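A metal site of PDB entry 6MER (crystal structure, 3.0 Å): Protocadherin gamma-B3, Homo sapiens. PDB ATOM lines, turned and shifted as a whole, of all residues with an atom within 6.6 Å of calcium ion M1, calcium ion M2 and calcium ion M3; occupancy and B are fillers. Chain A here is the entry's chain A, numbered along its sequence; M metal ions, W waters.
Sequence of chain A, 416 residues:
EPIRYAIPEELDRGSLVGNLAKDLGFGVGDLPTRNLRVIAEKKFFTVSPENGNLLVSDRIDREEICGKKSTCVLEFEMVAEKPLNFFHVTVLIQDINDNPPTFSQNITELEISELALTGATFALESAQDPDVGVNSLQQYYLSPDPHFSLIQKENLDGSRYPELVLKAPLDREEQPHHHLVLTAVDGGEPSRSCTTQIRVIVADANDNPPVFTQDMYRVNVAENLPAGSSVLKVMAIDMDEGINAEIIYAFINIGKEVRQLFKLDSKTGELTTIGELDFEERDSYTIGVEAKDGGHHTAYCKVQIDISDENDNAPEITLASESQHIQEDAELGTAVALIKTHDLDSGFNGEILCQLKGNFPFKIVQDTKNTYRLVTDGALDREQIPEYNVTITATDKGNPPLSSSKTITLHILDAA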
ATOM      1  N   GLU A 223      12.831   0.931  -7.310  1.00  0.00           N
ATOM      2  CA  GLU A 223      12.828   1.566  -5.992  1.00  0.00           C
ATOM      3  C   GLU A 223      11.488   1.438  -5.285  1.00  0.00           C
ATOM      4  O   GLU A 223      11.437   1.532  -4.057  1.00  0.00           O
ATOM      5  CB  GLU A 223      13.229   3.040  -6.112  1.00  0.00           C
ATOM      6  CG  GLU A 223      12.418   3.826  -7.120  1.00  0.00           C
ATOM      7  CD  GLU A 223      12.837   5.277  -7.186  1.00  0.00           C
ATOM      8  OE1 GLU A 223      13.339   5.799  -6.170  1.00  0.00           O
ATOM      9  OE2 GLU A 223      12.666   5.898  -8.255  1.00  0.00           O
ATOM     10  N   LEU A 277      13.673   1.022  -0.715  1.00  0.00           N
ATOM     11  CA  LEU A 277      14.652   1.430  -1.706  1.00  0.00           C
ATOM     12  C   LEU A 277      14.322   2.812  -2.245  1.00  0.00           C
ATOM     13  O   LEU A 277      13.157   3.183  -2.379  1.00  0.00           O
ATOM     14  CB  LEU A 277      14.706   0.415  -2.859  1.00  0.00           C
ATOM     15  CG  LEU A 277      15.160  -1.020  -2.571  1.00  0.00           C
ATOM     16  CD1 LEU A 277      16.336  -1.040  -1.591  1.00  0.00           C
ATOM     17  CD2 LEU A 277      14.012  -1.885  -2.058  1.00  0.00           C
ATOM     18  N   ASP A 278      15.374   3.576  -2.560  1.00  0.00           N
ATOM     19  CA  ASP A 278      15.216   4.927  -3.092  1.00  0.00           C
ATOM     20  C   ASP A 278      16.330   5.168  -4.104  1.00  0.00           C
ATOM     21  O   ASP A 278      17.502   5.204  -3.731  1.00  0.00           O
ATOM     22  CB  ASP A 278      15.245   5.966  -1.976  1.00  0.00           C
ATOM     23  CG  ASP A 278      14.821   7.341  -2.457  1.00  0.00           C
ATOM     24  OD1 ASP A 278      13.646   7.511  -2.833  1.00  0.00           O
ATOM     25  OD2 ASP A 278      15.665   8.259  -2.452  1.00  0.00           O
ATOM     26  N   PHE A 279      15.949   5.324  -5.379  1.00  0.00           N
ATOM     27  CA  PHE A 279      16.939   5.587  -6.413  1.00  0.00           C
ATOM     28  C   PHE A 279      17.616   6.944  -6.221  1.00  0.00           C
ATOM     29  O   PHE A 279      18.757   7.133  -6.648  1.00  0.00           O
ATOM     30  CB  PHE A 279      16.284   5.504  -7.792  1.00  0.00           C
ATOM     31  CG  PHE A 279      17.233   5.711  -8.935  1.00  0.00           C
ATOM     32  CD1 PHE A 279      18.002   4.667  -9.402  1.00  0.00           C
ATOM     33  CD2 PHE A 279      17.347   6.952  -9.543  1.00  0.00           C
ATOM     34  CE1 PHE A 279      18.879   4.850 -10.467  1.00  0.00           C
ATOM     35  CE2 PHE A 279      18.216   7.145 -10.601  1.00  0.00           C
ATOM     36  CZ  PHE A 279      18.980   6.088 -11.058  1.00  0.00           C
ATOM     37  N   GLU A 280      16.912   7.897  -5.590  1.00  0.00           N
ATOM     38  CA  GLU A 280      17.497   9.210  -5.362  1.00  0.00           C
ATOM     39  C   GLU A 280      18.538   9.209  -4.250  1.00  0.00           C
ATOM     40  O   GLU A 280      19.403  10.092  -4.230  1.00  0.00           O
ATOM     41  CB  GLU A 280      16.394  10.226  -5.052  1.00  0.00           C
ATOM     42  CG  GLU A 280      15.609  10.699  -6.268  1.00  0.00           C
ATOM     43  CD  GLU A 280      14.769   9.592  -6.889  1.00  0.00           C
ATOM     44  OE1 GLU A 280      14.372   8.657  -6.161  1.00  0.00           O
ATOM     45  OE2 GLU A 280      14.501   9.666  -8.105  1.00  0.00           O
ATOM     46  N   GLU A 281      18.474   8.244  -3.332  1.00  0.00           N
ATOM     47  CA  GLU A 281      19.438   8.161  -2.247  1.00  0.00           C
ATOM     48  C   GLU A 281      20.648   7.321  -2.637  1.00  0.00           C
ATOM     49  O   GLU A 281      21.792   7.746  -2.428  1.00  0.00           O
ATOM     50  CB  GLU A 281      18.766   7.576  -0.998  1.00  0.00           C
ATOM     51  CG  GLU A 281      19.686   7.466   0.218  1.00  0.00           C
ATOM     52  CD  GLU A 281      20.019   8.806   0.838  1.00  0.00           C
ATOM     53  OE1 GLU A 281      19.345   9.811   0.508  1.00  0.00           O
ATOM     54  OE2 GLU A 281      20.960   8.869   1.648  1.00  0.00           O
ATOM     55  N   SER A 308      16.339   0.620 -10.359  1.00  0.00           N
ATOM     56  CA  SER A 308      15.799   1.386 -11.477  1.00  0.00           C
ATOM     57  C   SER A 308      15.040   2.606 -10.970  1.00  0.00           C
ATOM     58  O   SER A 308      14.440   2.579  -9.892  1.00  0.00           O
ATOM     59  CB  SER A 308      14.883   0.511 -12.334  1.00  0.00           C
ATOM     60  OG  SER A 308      15.576  -0.596 -12.871  1.00  0.00           O
ATOM     61  N   ASP A 309      15.084   3.666 -11.761  1.00  0.00           N
ATOM     62  CA  ASP A 309      14.418   4.914 -11.399  1.00  0.00           C
ATOM     63  C   ASP A 309      12.922   4.810 -11.713  1.00  0.00           C
ATOM     64  O   ASP A 309      12.546   4.589 -12.868  1.00  0.00           O
ATOM     65  CB  ASP A 309      15.042   6.095 -12.136  1.00  0.00           C
ATOM     66  CG  ASP A 309      14.467   7.428 -11.718  1.00  0.00           C
ATOM     67  OD1 ASP A 309      13.840   7.494 -10.638  1.00  0.00           O
ATOM     68  OD2 ASP A 309      14.637   8.410 -12.468  1.00  0.00           O
ATOM     69  N   GLU A 310      12.093   4.972 -10.689  1.00  0.00           N
ATOM     70  CA  GLU A 310      10.648   5.038 -10.859  1.00  0.00           C
ATOM     71  C   GLU A 310      10.177   6.482 -10.732  1.00  0.00           C
ATOM     72  O   GLU A 310      10.766   7.281 -10.002  1.00  0.00           O
ATOM     73  CB  GLU A 310       9.940   4.155  -9.829  1.00  0.00           C
ATOM     74  CG  GLU A 310       9.985   2.672 -10.138  1.00  0.00           C
ATOM     75  CD  GLU A 310       9.108   2.286 -11.306  1.00  0.00           C
ATOM     76  OE1 GLU A 310       8.221   3.078 -11.685  1.00  0.00           O
ATOM     77  OE2 GLU A 310       9.299   1.180 -11.860  1.00  0.00           O
ATOM     78  N   ASN A 311       9.105   6.805 -11.446  1.00  0.00           N
ATOM     79  CA  ASN A 311       8.543   8.151 -11.447  1.00  0.00           C
ATOM     80  C   ASN A 311       7.678   8.346 -10.199  1.00  0.00           C
ATOM     81  O   ASN A 311       6.453   8.402 -10.244  1.00  0.00           O
ATOM     82  CB  ASN A 311       7.755   8.409 -12.716  1.00  0.00           C
ATOM     83  CG  ASN A 311       7.455   9.873 -12.939  1.00  0.00           C
ATOM     84  OD1 ASN A 311       8.231  10.746 -12.540  1.00  0.00           O
ATOM     85  ND2 ASN A 311       6.325  10.170 -13.571  1.00  0.00           N
ATOM     86  N   ASP A 312       8.357   8.451  -9.058  1.00  0.00           N
ATOM     87  CA  ASP A 312       7.707   8.624  -7.765  1.00  0.00           C
ATOM     88  C   ASP A 312       7.908  10.011  -7.181  1.00  0.00           C
ATOM     89  O   ASP A 312       7.626  10.230  -5.998  1.00  0.00           O
ATOM     90  CB  ASP A 312       8.190   7.552  -6.776  1.00  0.00           C
ATOM     91  CG  ASP A 312       9.704   7.522  -6.643  1.00  0.00           C
ATOM     92  OD1 ASP A 312      10.381   8.336  -7.318  1.00  0.00           O
ATOM     93  OD2 ASP A 312      10.208   6.683  -5.872  1.00  0.00           O
ATOM     94  N   ASN A 313       8.403  10.965  -7.978  1.00  0.00           N
ATOM     95  CA  ASN A 313       8.586  12.335  -7.540  1.00  0.00           C
ATOM     96  C   ASN A 313       7.931  13.278  -8.553  1.00  0.00           C
ATOM     97  O   ASN A 313       8.187  13.157  -9.755  1.00  0.00           O
ATOM     98  CB  ASN A 313      10.071  12.679  -7.377  1.00  0.00           C
ATOM     99  CG  ASN A 313      10.651  12.129  -6.086  1.00  0.00           C
ATOM    100  OD1 ASN A 313      10.664  12.810  -5.065  1.00  0.00           O
ATOM    101  ND2 ASN A 313      11.138  10.901  -6.132  1.00  0.00           N
ATOM    102  N   ALA A 314       7.107  14.186  -8.057  1.00  0.00           N
ATOM    103  CA  ALA A 314       6.433  15.149  -8.929  1.00  0.00           C
ATOM    104  C   ALA A 314       7.258  16.426  -9.053  1.00  0.00           C
ATOM    105  O   ALA A 314       7.919  16.839  -8.089  1.00  0.00           O
ATOM    106  CB  ALA A 314       5.051  15.490  -8.381  1.00  0.00           C
ATOM    107  N   PRO A 315       7.248  17.062 -10.225  1.00  0.00           N
ATOM    108  CA  PRO A 315       8.012  18.305 -10.408  1.00  0.00           C
ATOM    109  C   PRO A 315       7.414  19.430  -9.569  1.00  0.00           C
ATOM    110  O   PRO A 315       6.242  19.760  -9.698  1.00  0.00           O
ATOM    111  CB  PRO A 315       7.881  18.590 -11.906  1.00  0.00           C
ATOM    112  CG  PRO A 315       7.435  17.296 -12.525  1.00  0.00           C
ATOM    113  CD  PRO A 315       6.604  16.620 -11.470  1.00  0.00           C
ATOM    114  N   ASP A 343      12.990  18.173 -11.066  1.00  0.00           N
ATOM    115  CA  ASP A 343      12.427  16.885 -10.687  1.00  0.00           C
ATOM    116  C   ASP A 343      13.549  15.997 -10.166  1.00  0.00           C
ATOM    117  O   ASP A 343      14.594  15.863 -10.822  1.00  0.00           O
ATOM    118  CB  ASP A 343      11.719  16.225 -11.863  1.00  0.00           C
ATOM    119  CG  ASP A 343      10.833  15.079 -11.443  1.00  0.00           C
ATOM    120  OD1 ASP A 343       9.655  15.324 -11.105  1.00  0.00           O
ATOM    121  OD2 ASP A 343      11.307  13.923 -11.440  1.00  0.00           O
ATOM    122  N   LEU A 344      13.346  15.403  -8.989  1.00  0.00           N
ATOM    123  CA  LEU A 344      14.393  14.607  -8.360  1.00  0.00           C
ATOM    124  C   LEU A 344      14.720  13.342  -9.152  1.00  0.00           C
ATOM    125  O   LEU A 344      15.828  12.820  -9.016  1.00  0.00           O
ATOM    126  CB  LEU A 344      13.986  14.236  -6.939  1.00  0.00           C
ATOM    127  CG  LEU A 344      13.687  15.402  -5.991  1.00  0.00           C
ATOM    128  CD1 LEU A 344      13.415  14.893  -4.583  1.00  0.00           C
ATOM    129  CD2 LEU A 344      14.831  16.411  -6.003  1.00  0.00           C
ATOM    130  N   ASP A 345      13.798  12.860  -9.975  1.00  0.00           N
ATOM    131  CA  ASP A 345      14.048  11.668 -10.755  1.00  0.00           C
ATOM    132  C   ASP A 345      15.029  11.965 -11.891  1.00  0.00           C
ATOM    133  O   ASP A 345      15.267  13.124 -12.261  1.00  0.00           O
ATOM    134  CB  ASP A 345      12.749  11.110 -11.333  1.00  0.00           C
ATOM    135  CG  ASP A 345      11.663  10.975 -10.298  1.00  0.00           C
ATOM    136  OD1 ASP A 345      11.991  10.671  -9.125  1.00  0.00           O
ATOM    137  OD2 ASP A 345      10.473  11.168 -10.637  1.00  0.00           O
ATOM    138  N   SER A 346      15.617  10.905 -12.431  1.00  0.00           N
ATOM    139  CA  SER A 346      16.575  11.008 -13.523  1.00  0.00           C
ATOM    140  C   SER A 346      15.926  10.583 -14.843  1.00  0.00           C
ATOM    141  O   SER A 346      14.778  10.121 -14.886  1.00  0.00           O
ATOM    142  CB  SER A 346      17.811  10.157 -13.237  1.00  0.00           C
ATOM    143  OG  SER A 346      18.430  10.547 -12.026  1.00  0.00           O
ATOM    144  N   PHE A 348      14.137  10.629 -18.466  1.00  0.00           N
ATOM    145  CA  PHE A 348      12.941  11.340 -18.912  1.00  0.00           C
ATOM    146  C   PHE A 348      11.956  11.565 -17.768  1.00  0.00           C
ATOM    147  O   PHE A 348      11.066  12.413 -17.899  1.00  0.00           O
ATOM    148  CB  PHE A 348      12.259  10.577 -20.047  1.00  0.00           C
ATOM    149  CG  PHE A 348      12.897  10.794 -21.384  1.00  0.00           C
ATOM    150  CD1 PHE A 348      12.554  11.892 -22.161  1.00  0.00           C
ATOM    151  CD2 PHE A 348      13.844   9.910 -21.880  1.00  0.00           C
ATOM    152  CE1 PHE A 348      13.135  12.108 -23.388  1.00  0.00           C
ATOM    153  CE2 PHE A 348      14.433  10.117 -23.114  1.00  0.00           C
ATOM    154  CZ  PHE A 348      14.076  11.212 -23.873  1.00  0.00           C
ATOM    155  N   ASN A 349      12.094  10.825 -16.666  1.00  0.00           N
ATOM    156  CA  ASN A 349      11.264  11.098 -15.497  1.00  0.00           C
ATOM    157  C   ASN A 349      11.596  12.434 -14.855  1.00  0.00           C
ATOM    158  O   ASN A 349      10.787  12.960 -14.083  1.00  0.00           O
ATOM    159  CB  ASN A 349      11.435   9.981 -14.462  1.00  0.00           C
ATOM    160  CG  ASN A 349      11.102   8.606 -15.021  1.00  0.00           C
ATOM    161  OD1 ASN A 349      10.130   8.444 -15.749  1.00  0.00           O
ATOM    162  ND2 ASN A 349      11.925   7.622 -14.682  1.00  0.00           N
ATOM    163  N   GLY A 350      12.759  13.007 -15.172  1.00  0.00           N
ATOM    164  CA  GLY A 350      13.176  14.270 -14.593  1.00  0.00           C
ATOM    165  C   GLY A 350      12.979  15.455 -15.516  1.00  0.00           C
ATOM    166  O   GLY A 350      12.927  16.597 -15.060  1.00  0.00           O
ATOM    167  N   GLU A 351      12.854  15.203 -16.820  1.00  0.00           N
ATOM    168  CA  GLU A 351      12.587  16.273 -17.760  1.00  0.00           C
ATOM    169  C   GLU A 351      11.176  16.818 -17.561  1.00  0.00           C
ATOM    170  O   GLU A 351      10.225  16.053 -17.402  1.00  0.00           O
ATOM    171  CB  GLU A 351      12.776  15.799 -19.203  1.00  0.00           C
ATOM    172  CG  GLU A 351      14.225  15.505 -19.566  1.00  0.00           C
ATOM    173  CD  GLU A 351      14.415  15.320 -21.061  1.00  0.00           C
ATOM    174  OE1 GLU A 351      13.442  15.503 -21.816  1.00  0.00           O
ATOM    175  OE2 GLU A 351      15.553  15.006 -21.488  1.00  0.00           O
ATOM    176  N   ASP A 396       6.053  16.221 -15.917  1.00  0.00           N
ATOM    177  CA  ASP A 396       7.241  15.496 -16.358  1.00  0.00           C
ATOM    178  C   ASP A 396       6.911  14.603 -17.546  1.00  0.00           C
ATOM    179  O   ASP A 396       5.750  14.436 -17.935  1.00  0.00           O
ATOM    180  CB  ASP A 396       7.825  14.689 -15.203  1.00  0.00           C
ATOM    181  CG  ASP A 396       6.817  13.744 -14.554  1.00  0.00           C
ATOM    182  OD1 ASP A 396       5.733  13.534 -15.131  1.00  0.00           O
ATOM    183  OD2 ASP A 396       7.115  13.235 -13.464  1.00  0.00           O
ATOM    184  N   LYS A 397       7.961  14.022 -18.134  1.00  0.00           N
ATOM    185  CA  LYS A 397       7.816  13.166 -19.305  1.00  0.00           C
ATOM    186  C   LYS A 397       7.951  11.685 -18.967  1.00  0.00           C
ATOM    187  O   LYS A 397       8.346  10.881 -19.815  1.00  0.00           O
ATOM    188  CB  LYS A 397       8.852  13.555 -20.365  1.00  0.00           C
ATOM    189  CG  LYS A 397       8.723  15.002 -20.830  1.00  0.00           C
ATOM    190  CD  LYS A 397       9.783  15.335 -21.870  1.00  0.00           C
ATOM    191  CE  LYS A 397       9.658  16.780 -22.326  1.00  0.00           C
ATOM    192  NZ  LYS A 397      10.674  17.115 -23.367  1.00  0.00           N
ATOM    193  N   GLY A 398       7.635  11.307 -17.722  1.00  0.00           N
ATOM    194  CA  GLY A 398       7.731   9.931 -17.292  1.00  0.00           C
ATOM    195  C   GLY A 398       6.490   9.125 -17.605  1.00  0.00           C
ATOM    196  O   GLY A 398       5.589   9.562 -18.321  1.00  0.00           O
ATOM    197  N   LEU A 402       3.581  12.643 -13.899  1.00  0.00           N
ATOM    198  CA  LEU A 402       3.101  13.371 -12.738  1.00  0.00           C
ATOM    199  C   LEU A 402       3.247  14.876 -12.983  1.00  0.00           C
ATOM    200  O   LEU A 402       4.073  15.311 -13.785  1.00  0.00           O
ATOM    201  CB  LEU A 402       3.864  12.979 -11.466  1.00  0.00           C
ATOM    202  CG  LEU A 402       3.759  11.514 -11.046  1.00  0.00           C
ATOM    203  CD1 LEU A 402       4.577  11.254  -9.781  1.00  0.00           C
ATOM    204  CD2 LEU A 402       2.304  11.121 -10.821  1.00  0.00           C
HETATM  205 CA    CA M   1      12.540   8.319  -8.577  1.00  0.00          CA
HETATM  206 CA    CA M   2       9.146  12.976 -11.995  1.00  0.00          CA
HETATM  207 CA    CA M   3      12.316   7.803  -4.979  1.00  0.00          CA
HETATM  208  O   HOH W   1       9.875   9.496  -3.481  1.00  0.00           O
HETATM  209  O   HOH W   2      11.428   5.977  -3.416  1.00  0.00           O
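Calcium ion M3 is bound by the side-chain carboxylate of Glu 280, the side-chain carboxylate of Asp 278, the side-chain carboxylate of Glu 223, the side-chain carboxylate of Asp 312 and water W2. Slightly farther from calcium ion M3 lies the side-chain carboxylate (OD1) of Asp 312 (3.1 Å).
Water W1 lies within hydrogen-bond range of the side-chain amide nitrogen of Asn 313 (3.3 Å) and the backbone carbonyl oxygen of Asp 312 (3.5 Å).
Within 4 Å of calcium ion M3: Glu 223, Asp 278, Glu 280, Asp 312 and Asn 313.
Seven residues have an atom within 4 Å of calcium ion M1: Glu 223, Glu 280, Asp 309, Glu 310, Asp 312, Asn 313 and Asp 345.
The side-chain carboxylate (OD2) of Asp 343 is bound to calcium ion M2 (2.4 Å). O of Asn 313 is bound to calcium ion M2 (2.4 Å). The side-chain amide oxygen (OD1) of Asn 311 binds calcium ion M2 (2.5 Å). OD2 of Asp 396 binds calcium ion M2, at 2.5 Å. OD1 of Asp 343 binds calcium ion M2 (2.6 Å). OD2 of Asp 345 is bound to calcium ion M2, at 2.6 Å. Calcium ion M2 is bound by O of Asn 349, 2.7 Å away.
Calcium ion M1 is bound by OE2 of Glu 280. OE2 of Glu 223 is bound to calcium ion M1 (2.4 Å). OD1 of Asp 345 is bound to calcium ion M1, at 2.5 Å. Calcium ion M1 is bound by OD1 of Asp 312, at 2.5 Å. O of Glu 310 is bound to calcium ion M1 (2.5 Å). OD1 of Asp 309 is bound to calcium ion M1 (2.6 Å). Slightly farther from calcium ion M1 lies OE1 of Glu 280 (3.1 Å).
Within 4 Å of calcium ion M2: Asn 311, Asn 313, Asp 343, Asp 345, Asn 349 and Asp 396. The nearest printed residue that does not touch calcium ion M2 is Pro 315 (4.5 Å).
OD2 of Asp 309 is in hydrogen-bond range of N of Ser 346 (2.7 Å). The side-chain carboxylate (OD1) of Asp 396 is in hydrogen-bond range of the backbone NH (N) of Leu 402, at 2.6 Å. The backbone NH of Glu 223 lies within hydrogen-bond range of the backbone carbonyl oxygen of Ser 308. The backbone NH (N) of Glu 281 is in hydrogen-bond range of the side-chain carboxylate (OD2) of Asp 278 (2.9 Å). The side-chain carboxylate of Glu 223 lies close to the backbone NH of Phe 279 (2.8 Å). The side-chain amide nitrogen (ND2) of Asn 313 lies close to the side-chain carboxylate (OD1) of Asp 312 (2.9 Å).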
